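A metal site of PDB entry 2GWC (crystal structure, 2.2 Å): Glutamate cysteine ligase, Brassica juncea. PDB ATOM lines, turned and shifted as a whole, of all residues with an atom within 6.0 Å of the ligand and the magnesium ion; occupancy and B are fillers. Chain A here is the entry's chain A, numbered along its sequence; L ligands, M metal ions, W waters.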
ATOM      1  N   GLU A  40      -7.709  33.140  -0.488  1.00  0.00           N
ATOM      2  CA  GLU A  40      -6.437  32.560  -0.950  1.00  0.00           C
ATOM      3  C   GLU A  40      -6.414  32.596  -2.495  1.00  0.00           C
ATOM      4  O   GLU A  40      -7.405  32.404  -3.119  1.00  0.00           O
ATOM      5  CB  GLU A  40      -6.239  31.113  -0.515  1.00  0.00           C
ATOM      6  CG  GLU A  40      -6.583  30.767   0.962  1.00  0.00           C
ATOM      7  CD  GLU A  40      -6.446  29.263   1.258  1.00  0.00           C
ATOM      8  OE1 GLU A  40      -5.694  28.576   0.526  1.00  0.00           O
ATOM      9  OE2 GLU A  40      -7.148  28.770   2.215  1.00  0.00           O
ATOM     10  N   GLU A  42      -3.560  31.621  -6.030  1.00  0.00           N
ATOM     11  CA  GLU A  42      -2.302  31.130  -6.530  1.00  0.00           C
ATOM     12  C   GLU A  42      -2.012  31.768  -7.905  1.00  0.00           C
ATOM     13  O   GLU A  42      -2.944  32.057  -8.693  1.00  0.00           O
ATOM     14  CB  GLU A  42      -2.385  29.610  -6.656  1.00  0.00           C
ATOM     15  CG  GLU A  42      -2.981  28.881  -5.412  1.00  0.00           C
ATOM     16  CD  GLU A  42      -3.447  27.486  -5.675  1.00  0.00           C
ATOM     17  OE1 GLU A  42      -3.794  27.130  -6.836  1.00  0.00           O
ATOM     18  OE2 GLU A  42      -3.519  26.720  -4.684  1.00  0.00           O
ATOM     19  N   GLU A  94       2.809  26.044  -4.178  1.00  0.00           N
ATOM     20  CA  GLU A  94       2.166  24.824  -4.642  1.00  0.00           C
ATOM     21  C   GLU A  94       3.235  23.927  -5.296  1.00  0.00           C
ATOM     22  O   GLU A  94       4.417  24.343  -5.436  1.00  0.00           O
ATOM     23  CB  GLU A  94       1.005  25.140  -5.605  1.00  0.00           C
ATOM     24  CG  GLU A  94      -0.173  25.826  -4.921  1.00  0.00           C
ATOM     25  CD  GLU A  94      -0.989  24.902  -4.019  1.00  0.00           C
ATOM     26  OE1 GLU A  94      -0.805  23.697  -4.076  1.00  0.00           O
ATOM     27  OE2 GLU A  94      -1.837  25.373  -3.261  1.00  0.00           O
ATOM     28  N   PRO A  95       2.855  22.688  -5.639  1.00  0.00           N
ATOM     29  CA  PRO A  95       3.852  21.733  -6.158  1.00  0.00           C
ATOM     30  C   PRO A  95       4.662  22.176  -7.367  1.00  0.00           C
ATOM     31  O   PRO A  95       5.824  21.813  -7.485  1.00  0.00           O
ATOM     32  CB  PRO A  95       3.003  20.495  -6.480  1.00  0.00           C
ATOM     33  CG  PRO A  95       1.913  20.565  -5.482  1.00  0.00           C
ATOM     34  CD  PRO A  95       1.553  22.040  -5.472  1.00  0.00           C
ATOM     35  N   GLN A  98       3.678  27.442  -8.025  1.00  0.00           N
ATOM     36  CA  GLN A  98       2.627  28.462  -8.001  1.00  0.00           C
ATOM     37  C   GLN A  98       2.702  29.202  -6.659  1.00  0.00           C
ATOM     38  O   GLN A  98       2.819  28.615  -5.607  1.00  0.00           O
ATOM     39  CB  GLN A  98       1.237  27.874  -8.200  1.00  0.00           C
ATOM     40  CG  GLN A  98       1.096  26.965  -9.433  1.00  0.00           C
ATOM     41  CD  GLN A  98       1.177  25.479  -9.108  1.00  0.00           C
ATOM     42  OE1 GLN A  98       2.162  25.038  -8.553  1.00  0.00           O
ATOM     43  NE2 GLN A  98       0.136  24.720  -9.444  1.00  0.00           N
ATOM     44  N   GLU A 100       1.440  31.430  -3.796  1.00  0.00           N
ATOM     45  CA  GLU A 100       0.159  31.526  -3.109  1.00  0.00           C
ATOM     46  C   GLU A 100       0.140  32.523  -1.924  1.00  0.00           C
ATOM     47  O   GLU A 100       1.013  32.528  -1.100  1.00  0.00           O
ATOM     48  CB  GLU A 100      -0.250  30.133  -2.604  1.00  0.00           C
ATOM     49  CG  GLU A 100      -1.687  30.111  -2.043  1.00  0.00           C
ATOM     50  CD  GLU A 100      -2.085  28.811  -1.405  1.00  0.00           C
ATOM     51  OE1 GLU A 100      -2.300  27.810  -2.153  1.00  0.00           O
ATOM     52  OE2 GLU A 100      -2.230  28.779  -0.154  1.00  0.00           O
ATOM     53  N   GLY A 138      -6.142  29.855 -14.813  1.00  0.00           N
ATOM     54  CA  GLY A 138      -6.482  28.613 -14.126  1.00  0.00           C
ATOM     55  C   GLY A 138      -5.600  27.429 -14.454  1.00  0.00           C
ATOM     56  O   GLY A 138      -5.483  26.505 -13.635  1.00  0.00           O
ATOM     57  N   TYR A 156       4.664  16.962  -0.975  1.00  0.00           N
ATOM     58  CA  TYR A 156       4.380  16.877  -2.402  1.00  0.00           C
ATOM     59  C   TYR A 156       5.042  15.696  -3.076  1.00  0.00           C
ATOM     60  O   TYR A 156       4.522  15.219  -4.052  1.00  0.00           O
ATOM     61  CB  TYR A 156       4.780  18.167  -3.122  1.00  0.00           C
ATOM     62  CG  TYR A 156       4.027  19.386  -2.662  1.00  0.00           C
ATOM     63  CD1 TYR A 156       2.814  19.287  -1.997  1.00  0.00           C
ATOM     64  CD2 TYR A 156       4.539  20.652  -2.915  1.00  0.00           C
ATOM     65  CE1 TYR A 156       2.142  20.412  -1.582  1.00  0.00           C
ATOM     66  CE2 TYR A 156       3.836  21.796  -2.525  1.00  0.00           C
ATOM     67  CZ  TYR A 156       2.675  21.671  -1.859  1.00  0.00           C
ATOM     68  OH  TYR A 156       2.050  22.814  -1.474  1.00  0.00           O
ATOM     69  N   MET A 159       2.665  12.880  -2.449  1.00  0.00           N
ATOM     70  CA  MET A 159       1.497  13.070  -3.281  1.00  0.00           C
ATOM     71  C   MET A 159       1.743  12.772  -4.743  1.00  0.00           C
ATOM     72  O   MET A 159       0.898  12.166  -5.389  1.00  0.00           O
ATOM     73  CB  MET A 159       0.943  14.485  -3.134  1.00  0.00           C
ATOM     74  CG  MET A 159       0.351  14.735  -1.809  1.00  0.00           C
ATOM     75  SD  MET A 159      -0.298  16.609  -1.750  1.00  0.00           S
ATOM     76  CE  MET A 159      -1.670  16.567  -3.311  1.00  0.00           C
ATOM     77  N   MET A 163      -0.483  10.050  -6.871  1.00  0.00           N
ATOM     78  CA  MET A 163      -1.476  10.519  -7.853  1.00  0.00           C
ATOM     79  C   MET A 163      -1.753   9.574  -9.029  1.00  0.00           C
ATOM     80  O   MET A 163      -2.919   9.391  -9.402  1.00  0.00           O
ATOM     81  CB  MET A 163      -1.087  11.888  -8.414  1.00  0.00           C
ATOM     82  CG  MET A 163      -1.420  12.988  -7.502  1.00  0.00           C
ATOM     83  SD  MET A 163      -3.329  13.175  -6.969  1.00  0.00           S
ATOM     84  CE  MET A 163      -3.086  14.659  -5.616  1.00  0.00           C
ATOM     85  N   MET A 173      -3.246  18.752 -11.804  1.00  0.00           N
ATOM     86  CA  MET A 173      -3.778  19.537 -10.692  1.00  0.00           C
ATOM     87  C   MET A 173      -2.622  20.147  -9.857  1.00  0.00           C
ATOM     88  O   MET A 173      -2.587  21.341  -9.601  1.00  0.00           O
ATOM     89  CB  MET A 173      -4.700  18.663  -9.816  1.00  0.00           C
ATOM     90  CG  MET A 173      -5.359  19.375  -8.644  1.00  0.00           C
ATOM     91  SD  MET A 173      -4.149  19.588  -7.046  1.00  0.00           S
ATOM     92  CE  MET A 173      -4.178  17.659  -6.387  1.00  0.00           C
ATOM     93  N   MET A 174      -1.677  19.308  -9.474  1.00  0.00           N
ATOM     94  CA  MET A 174      -0.564  19.726  -8.607  1.00  0.00           C
ATOM     95  C   MET A 174       0.381  20.755  -9.248  1.00  0.00           C
ATOM     96  O   MET A 174       0.735  21.771  -8.617  1.00  0.00           O
ATOM     97  CB  MET A 174       0.256  18.502  -8.176  1.00  0.00           C
ATOM     98  CG  MET A 174      -0.504  17.578  -7.225  1.00  0.00           C
ATOM     99  SD  MET A 174       0.583  16.006  -6.759  1.00  0.00           S
ATOM    100  CE  MET A 174       1.873  16.911  -5.506  1.00  0.00           C
ATOM    101  N   THR A 177      -2.177  23.964 -12.265  1.00  0.00           N
ATOM    102  CA  THR A 177      -3.431  24.688 -12.004  1.00  0.00           C
ATOM    103  C   THR A 177      -3.264  25.803 -10.984  1.00  0.00           C
ATOM    104  O   THR A 177      -2.400  25.689 -10.124  1.00  0.00           O
ATOM    105  CB  THR A 177      -4.551  23.764 -11.454  1.00  0.00           C
ATOM    106  OG1 THR A 177      -4.109  23.148 -10.224  1.00  0.00           O
ATOM    107  CG2 THR A 177      -4.956  22.740 -12.493  1.00  0.00           C
ATOM    108  N   CYS A 178      -4.095  26.844 -11.086  1.00  0.00           N
ATOM    109  CA  CYS A 178      -4.178  27.929 -10.098  1.00  0.00           C
ATOM    110  C   CYS A 178      -5.625  28.290  -9.805  1.00  0.00           C
ATOM    111  O   CYS A 178      -6.463  28.412 -10.724  1.00  0.00           O
ATOM    112  CB  CYS A 178      -3.460  29.217 -10.572  1.00  0.00           C
ATOM    113  SG  CYS A 178      -1.682  29.244 -10.388  1.00  0.00           S
ATOM    114  N   THR A 179      -5.915  28.490  -8.526  1.00  0.00           N
ATOM    115  CA  THR A 179      -7.270  28.784  -8.050  1.00  0.00           C
ATOM    116  C   THR A 179      -7.311  30.134  -7.308  1.00  0.00           C
ATOM    117  O   THR A 179      -6.291  30.616  -6.824  1.00  0.00           O
ATOM    118  CB  THR A 179      -7.808  27.658  -7.077  1.00  0.00           C
ATOM    119  OG1 THR A 179      -9.111  28.003  -6.588  1.00  0.00           O
ATOM    120  CG2 THR A 179      -6.960  27.507  -5.883  1.00  0.00           C
ATOM    121  N   GLN A 181      -9.724  31.090  -4.033  1.00  0.00           N
ATOM    122  CA  GLN A 181     -10.757  30.586  -3.117  1.00  0.00           C
ATOM    123  C   GLN A 181     -11.103  31.527  -1.966  1.00  0.00           C
ATOM    124  O   GLN A 181     -10.368  32.469  -1.687  1.00  0.00           O
ATOM    125  CB  GLN A 181     -10.374  29.241  -2.571  1.00  0.00           C
ATOM    126  CG  GLN A 181      -9.182  29.190  -1.730  1.00  0.00           C
ATOM    127  CD  GLN A 181      -9.091  27.811  -1.117  1.00  0.00           C
ATOM    128  OE1 GLN A 181      -8.746  26.843  -1.820  1.00  0.00           O
ATOM    129  NE2 GLN A 181      -9.424  27.705   0.181  1.00  0.00           N
ATOM    130  N   ARG A 227      -8.884  23.368 -15.837  1.00  0.00           N
ATOM    131  CA  ARG A 227      -8.618  23.184 -14.418  1.00  0.00           C
ATOM    132  C   ARG A 227      -9.753  22.441 -13.690  1.00  0.00           C
ATOM    133  O   ARG A 227      -9.486  21.506 -12.967  1.00  0.00           O
ATOM    134  CB  ARG A 227      -8.390  24.516 -13.743  1.00  0.00           C
ATOM    135  CG  ARG A 227      -8.372  24.458 -12.218  1.00  0.00           C
ATOM    136  CD  ARG A 227      -8.317  25.869 -11.615  1.00  0.00           C
ATOM    137  NE  ARG A 227      -8.676  25.770 -10.231  1.00  0.00           N
ATOM    138  CZ  ARG A 227      -9.924  25.728  -9.782  1.00  0.00           C
ATOM    139  NH1 ARG A 227     -10.963  25.897 -10.586  1.00  0.00           N
ATOM    140  NH2 ARG A 227     -10.136  25.537  -8.492  1.00  0.00           N
ATOM    141  N   TRP A 231      -9.927  18.334 -12.004  1.00  0.00           N
ATOM    142  CA  TRP A 231     -10.442  17.884 -10.720  1.00  0.00           C
ATOM    143  C   TRP A 231     -11.431  16.731 -10.764  1.00  0.00           C
ATOM    144  O   TRP A 231     -11.744  16.187  -9.701  1.00  0.00           O
ATOM    145  CB  TRP A 231     -11.062  19.071  -9.970  1.00  0.00           C
ATOM    146  CG  TRP A 231     -10.059  19.948  -9.285  1.00  0.00           C
ATOM    147  CD1 TRP A 231      -9.710  21.228  -9.639  1.00  0.00           C
ATOM    148  CD2 TRP A 231      -9.270  19.633  -8.122  1.00  0.00           C
ATOM    149  NE1 TRP A 231      -8.772  21.720  -8.767  1.00  0.00           N
ATOM    150  CE2 TRP A 231      -8.512  20.778  -7.801  1.00  0.00           C
ATOM    151  CE3 TRP A 231      -9.170  18.514  -7.283  1.00  0.00           C
ATOM    152  CZ2 TRP A 231      -7.637  20.812  -6.705  1.00  0.00           C
ATOM    153  CZ3 TRP A 231      -8.328  18.544  -6.210  1.00  0.00           C
ATOM    154  CH2 TRP A 231      -7.561  19.686  -5.935  1.00  0.00           C
ATOM    155  N   THR A 307      -7.166  18.845   5.452  1.00  0.00           N
ATOM    156  CA  THR A 307      -6.582  19.668   4.395  1.00  0.00           C
ATOM    157  C   THR A 307      -6.131  18.854   3.166  1.00  0.00           C
ATOM    158  O   THR A 307      -5.693  19.434   2.170  1.00  0.00           O
ATOM    159  CB  THR A 307      -5.393  20.494   4.975  1.00  0.00           C
ATOM    160  OG1 THR A 307      -5.856  21.196   6.120  1.00  0.00           O
ATOM    161  CG2 THR A 307      -4.852  21.531   4.011  1.00  0.00           C
ATOM    162  N   PHE A 310     -10.440  17.287  -1.033  1.00  0.00           N
ATOM    163  CA  PHE A 310     -10.568  18.303  -2.118  1.00  0.00           C
ATOM    164  C   PHE A 310     -11.925  18.364  -2.831  1.00  0.00           C
ATOM    165  O   PHE A 310     -12.002  18.380  -4.074  1.00  0.00           O
ATOM    166  CB  PHE A 310      -9.461  18.107  -3.166  1.00  0.00           C
ATOM    167  CG  PHE A 310      -8.059  18.058  -2.581  1.00  0.00           C
ATOM    168  CD1 PHE A 310      -7.594  19.090  -1.776  1.00  0.00           C
ATOM    169  CD2 PHE A 310      -7.233  16.973  -2.820  1.00  0.00           C
ATOM    170  CE1 PHE A 310      -6.272  19.066  -1.229  1.00  0.00           C
ATOM    171  CE2 PHE A 310      -5.937  16.924  -2.267  1.00  0.00           C
ATOM    172  CZ  PHE A 310      -5.456  17.982  -1.472  1.00  0.00           C
ATOM    173  N   ARG A 314     -15.341  22.508   0.735  1.00  0.00           N
ATOM    174  CA  ARG A 314     -14.700  21.772   1.823  1.00  0.00           C
ATOM    175  C   ARG A 314     -15.118  22.304   3.199  1.00  0.00           C
ATOM    176  O   ARG A 314     -15.339  23.510   3.367  1.00  0.00           O
ATOM    177  CB  ARG A 314     -13.199  21.881   1.649  1.00  0.00           C
ATOM    178  CG  ARG A 314     -12.369  21.054   2.646  1.00  0.00           C
ATOM    179  CD  ARG A 314     -11.036  21.759   2.859  1.00  0.00           C
ATOM    180  NE  ARG A 314     -10.043  21.119   2.056  1.00  0.00           N
ATOM    181  CZ  ARG A 314      -8.797  21.551   1.894  1.00  0.00           C
ATOM    182  NH1 ARG A 314      -8.359  22.699   2.422  1.00  0.00           N
ATOM    183  NH2 ARG A 314      -8.012  20.815   1.132  1.00  0.00           N
ATOM    184  N   ARG A 322     -14.130  26.173  -3.484  1.00  0.00           N
ATOM    185  CA  ARG A 322     -12.899  25.778  -4.210  1.00  0.00           C
ATOM    186  C   ARG A 322     -13.027  25.685  -5.745  1.00  0.00           C
ATOM    187  O   ARG A 322     -12.112  25.225  -6.406  1.00  0.00           O
ATOM    188  CB  ARG A 322     -12.404  24.450  -3.641  1.00  0.00           C
ATOM    189  CG  ARG A 322     -12.057  24.475  -2.162  1.00  0.00           C
ATOM    190  CD  ARG A 322     -11.785  23.079  -1.640  1.00  0.00           C
ATOM    191  NE  ARG A 322     -10.905  22.333  -2.522  1.00  0.00           N
ATOM    192  CZ  ARG A 322      -9.564  22.387  -2.536  1.00  0.00           C
ATOM    193  NH1 ARG A 322      -8.871  23.101  -1.682  1.00  0.00           N
ATOM    194  NH2 ARG A 322      -8.925  21.640  -3.414  1.00  0.00           N
ATOM    195  N   ALA A 324     -13.314  27.983  -8.394  1.00  0.00           N
ATOM    196  CA  ALA A 324     -12.954  29.056  -9.341  1.00  0.00           C
ATOM    197  C   ALA A 324     -11.482  29.103  -9.752  1.00  0.00           C
ATOM    198  O   ALA A 324     -10.578  28.967  -8.912  1.00  0.00           O
ATOM    199  CB  ALA A 324     -13.343  30.418  -8.775  1.00  0.00           C
HETATM  200  C1  LIG L   1      -1.117  20.362  -3.498  1.00  0.00           C
HETATM  201  C2  LIG L   1      -2.622  20.133  -3.677  1.00  0.00           C
HETATM  202  C3  LIG L   1      -3.485  20.676  -2.554  1.00  0.00           C
HETATM  203  C4  LIG L   1      -3.520  22.202  -2.456  1.00  0.00           C
HETATM  204  S1  LIG L   1      -4.911  23.049  -3.293  1.00  0.00           S
HETATM  205  N1  LIG L   1      -6.265  22.297  -3.041  1.00  0.00           N
HETATM  206  O1  LIG L   1      -4.932  24.418  -2.720  1.00  0.00           O
HETATM  207  C5  LIG L   1      -4.520  23.223  -5.042  1.00  0.00           C
HETATM  208  C6  LIG L   1      -5.407  24.148  -5.799  1.00  0.00           C
HETATM  209  C7  LIG L   1      -5.111  23.950  -7.267  1.00  0.00           C
HETATM  210  C8  LIG L   1      -6.298  24.542  -7.992  1.00  0.00           C
HETATM  211  O2  LIG L   1      -6.029  25.303  -8.936  1.00  0.00           O
HETATM  212  O3  LIG L   1      -7.435  24.244  -7.569  1.00  0.00           O
HETATM  213  N2  LIG L   1      -3.840  24.600  -7.663  1.00  0.00           N
HETATM  214 MG    MG M   1      -3.610  26.411  -2.685  1.00  0.00          MG
HETATM  215  O   HOH W   1      -1.843  22.868  -6.919  1.00  0.00           O
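The guanidinium group (NH2) of Arg 322 sits close to a nitrogen (N1) of the ligand (2.8 Å).
The backbone carbonyl oxygen (O) of Thr 177 sits at hydrogen-bond distance from a nitrogen (N2) of the ligand (3.1 Å).
OG1 of Thr 177 sits at hydrogen-bond distance from N2 of the ligand (3.0 Å).
An oxygen (O2) of the ligand is in salt-bridge range of the guanidinium group of Arg 227, 3.0 Å away.
An oxygen (O3) of the ligand lies within hydrogen-bond range of the indole nitrogen of Trp 231, 3.1 Å away.
The backbone NH of Cys 178 lies close to an oxygen (O2) of the ligand, at 3.3 Å.
The backbone NH (N) of Thr 179 sits at hydrogen-bond distance from an oxygen (O2) of the ligand (3.2 Å).
O of Glu 42 lies close to SG of Cys 178, at 3.5 Å.
N of Glu 42 sits at hydrogen-bond distance from O of Thr 179 (3.0 Å).
The guanidinium group (NH2) of Arg 227 is in hydrogen-bond range of the backbone carbonyl oxygen (O) of Arg 322 (2.9 Å).
The side-chain hydroxyl of Thr 177 lies within hydrogen-bond range of the backbone carbonyl oxygen of Met 173 (2.4 Å).
NE of Arg 227 lies close to O of Cys 178 (3.5 Å).
The guanidinium group of Arg 227 lies within hydrogen-bond range of the side-chain hydroxyl of Thr 179, at 3.3 Å.
N of Cys 178 sits at hydrogen-bond distance from O of Gly 138 (2.9 Å).
The side-chain hydroxyl of Thr 179 lies within hydrogen-bond range of the backbone carbonyl oxygen of Ala 324 (2.9 Å).
Merely in contact with the ligand: Pro 95 (3.6 Å), Tyr 156 (3.8 Å), Met 159 (3.7 Å), Met 173 (3.7 Å) and Phe 310 (3.5 Å).
Hydrophobic or aromatic side chains within 4 Å of the ligand: Pro 95, Tyr 156, Met 159, Met 173, Trp 231 and Phe 310.
Within 4 Å of the ligand: Glu 42, Glu 94, Pro 95, Tyr 156, Met 159, Met 173, Thr 177, Cys 178, Thr 179, Arg 227, Trp 231, Phe 310 and Arg 322.
Within 4 Å of the magnesium ion: Glu 42, Glu 94 and Glu 100.
The magnesium ion is bound by OE1 of Glu 100 (2.0 Å), OE2 of Glu 42 (2.0 Å), OE2 of Glu 94 (2.1 Å) and O1 of the ligand (2.4 Å).
The magnesium ion has four donor atoms within binding distance.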
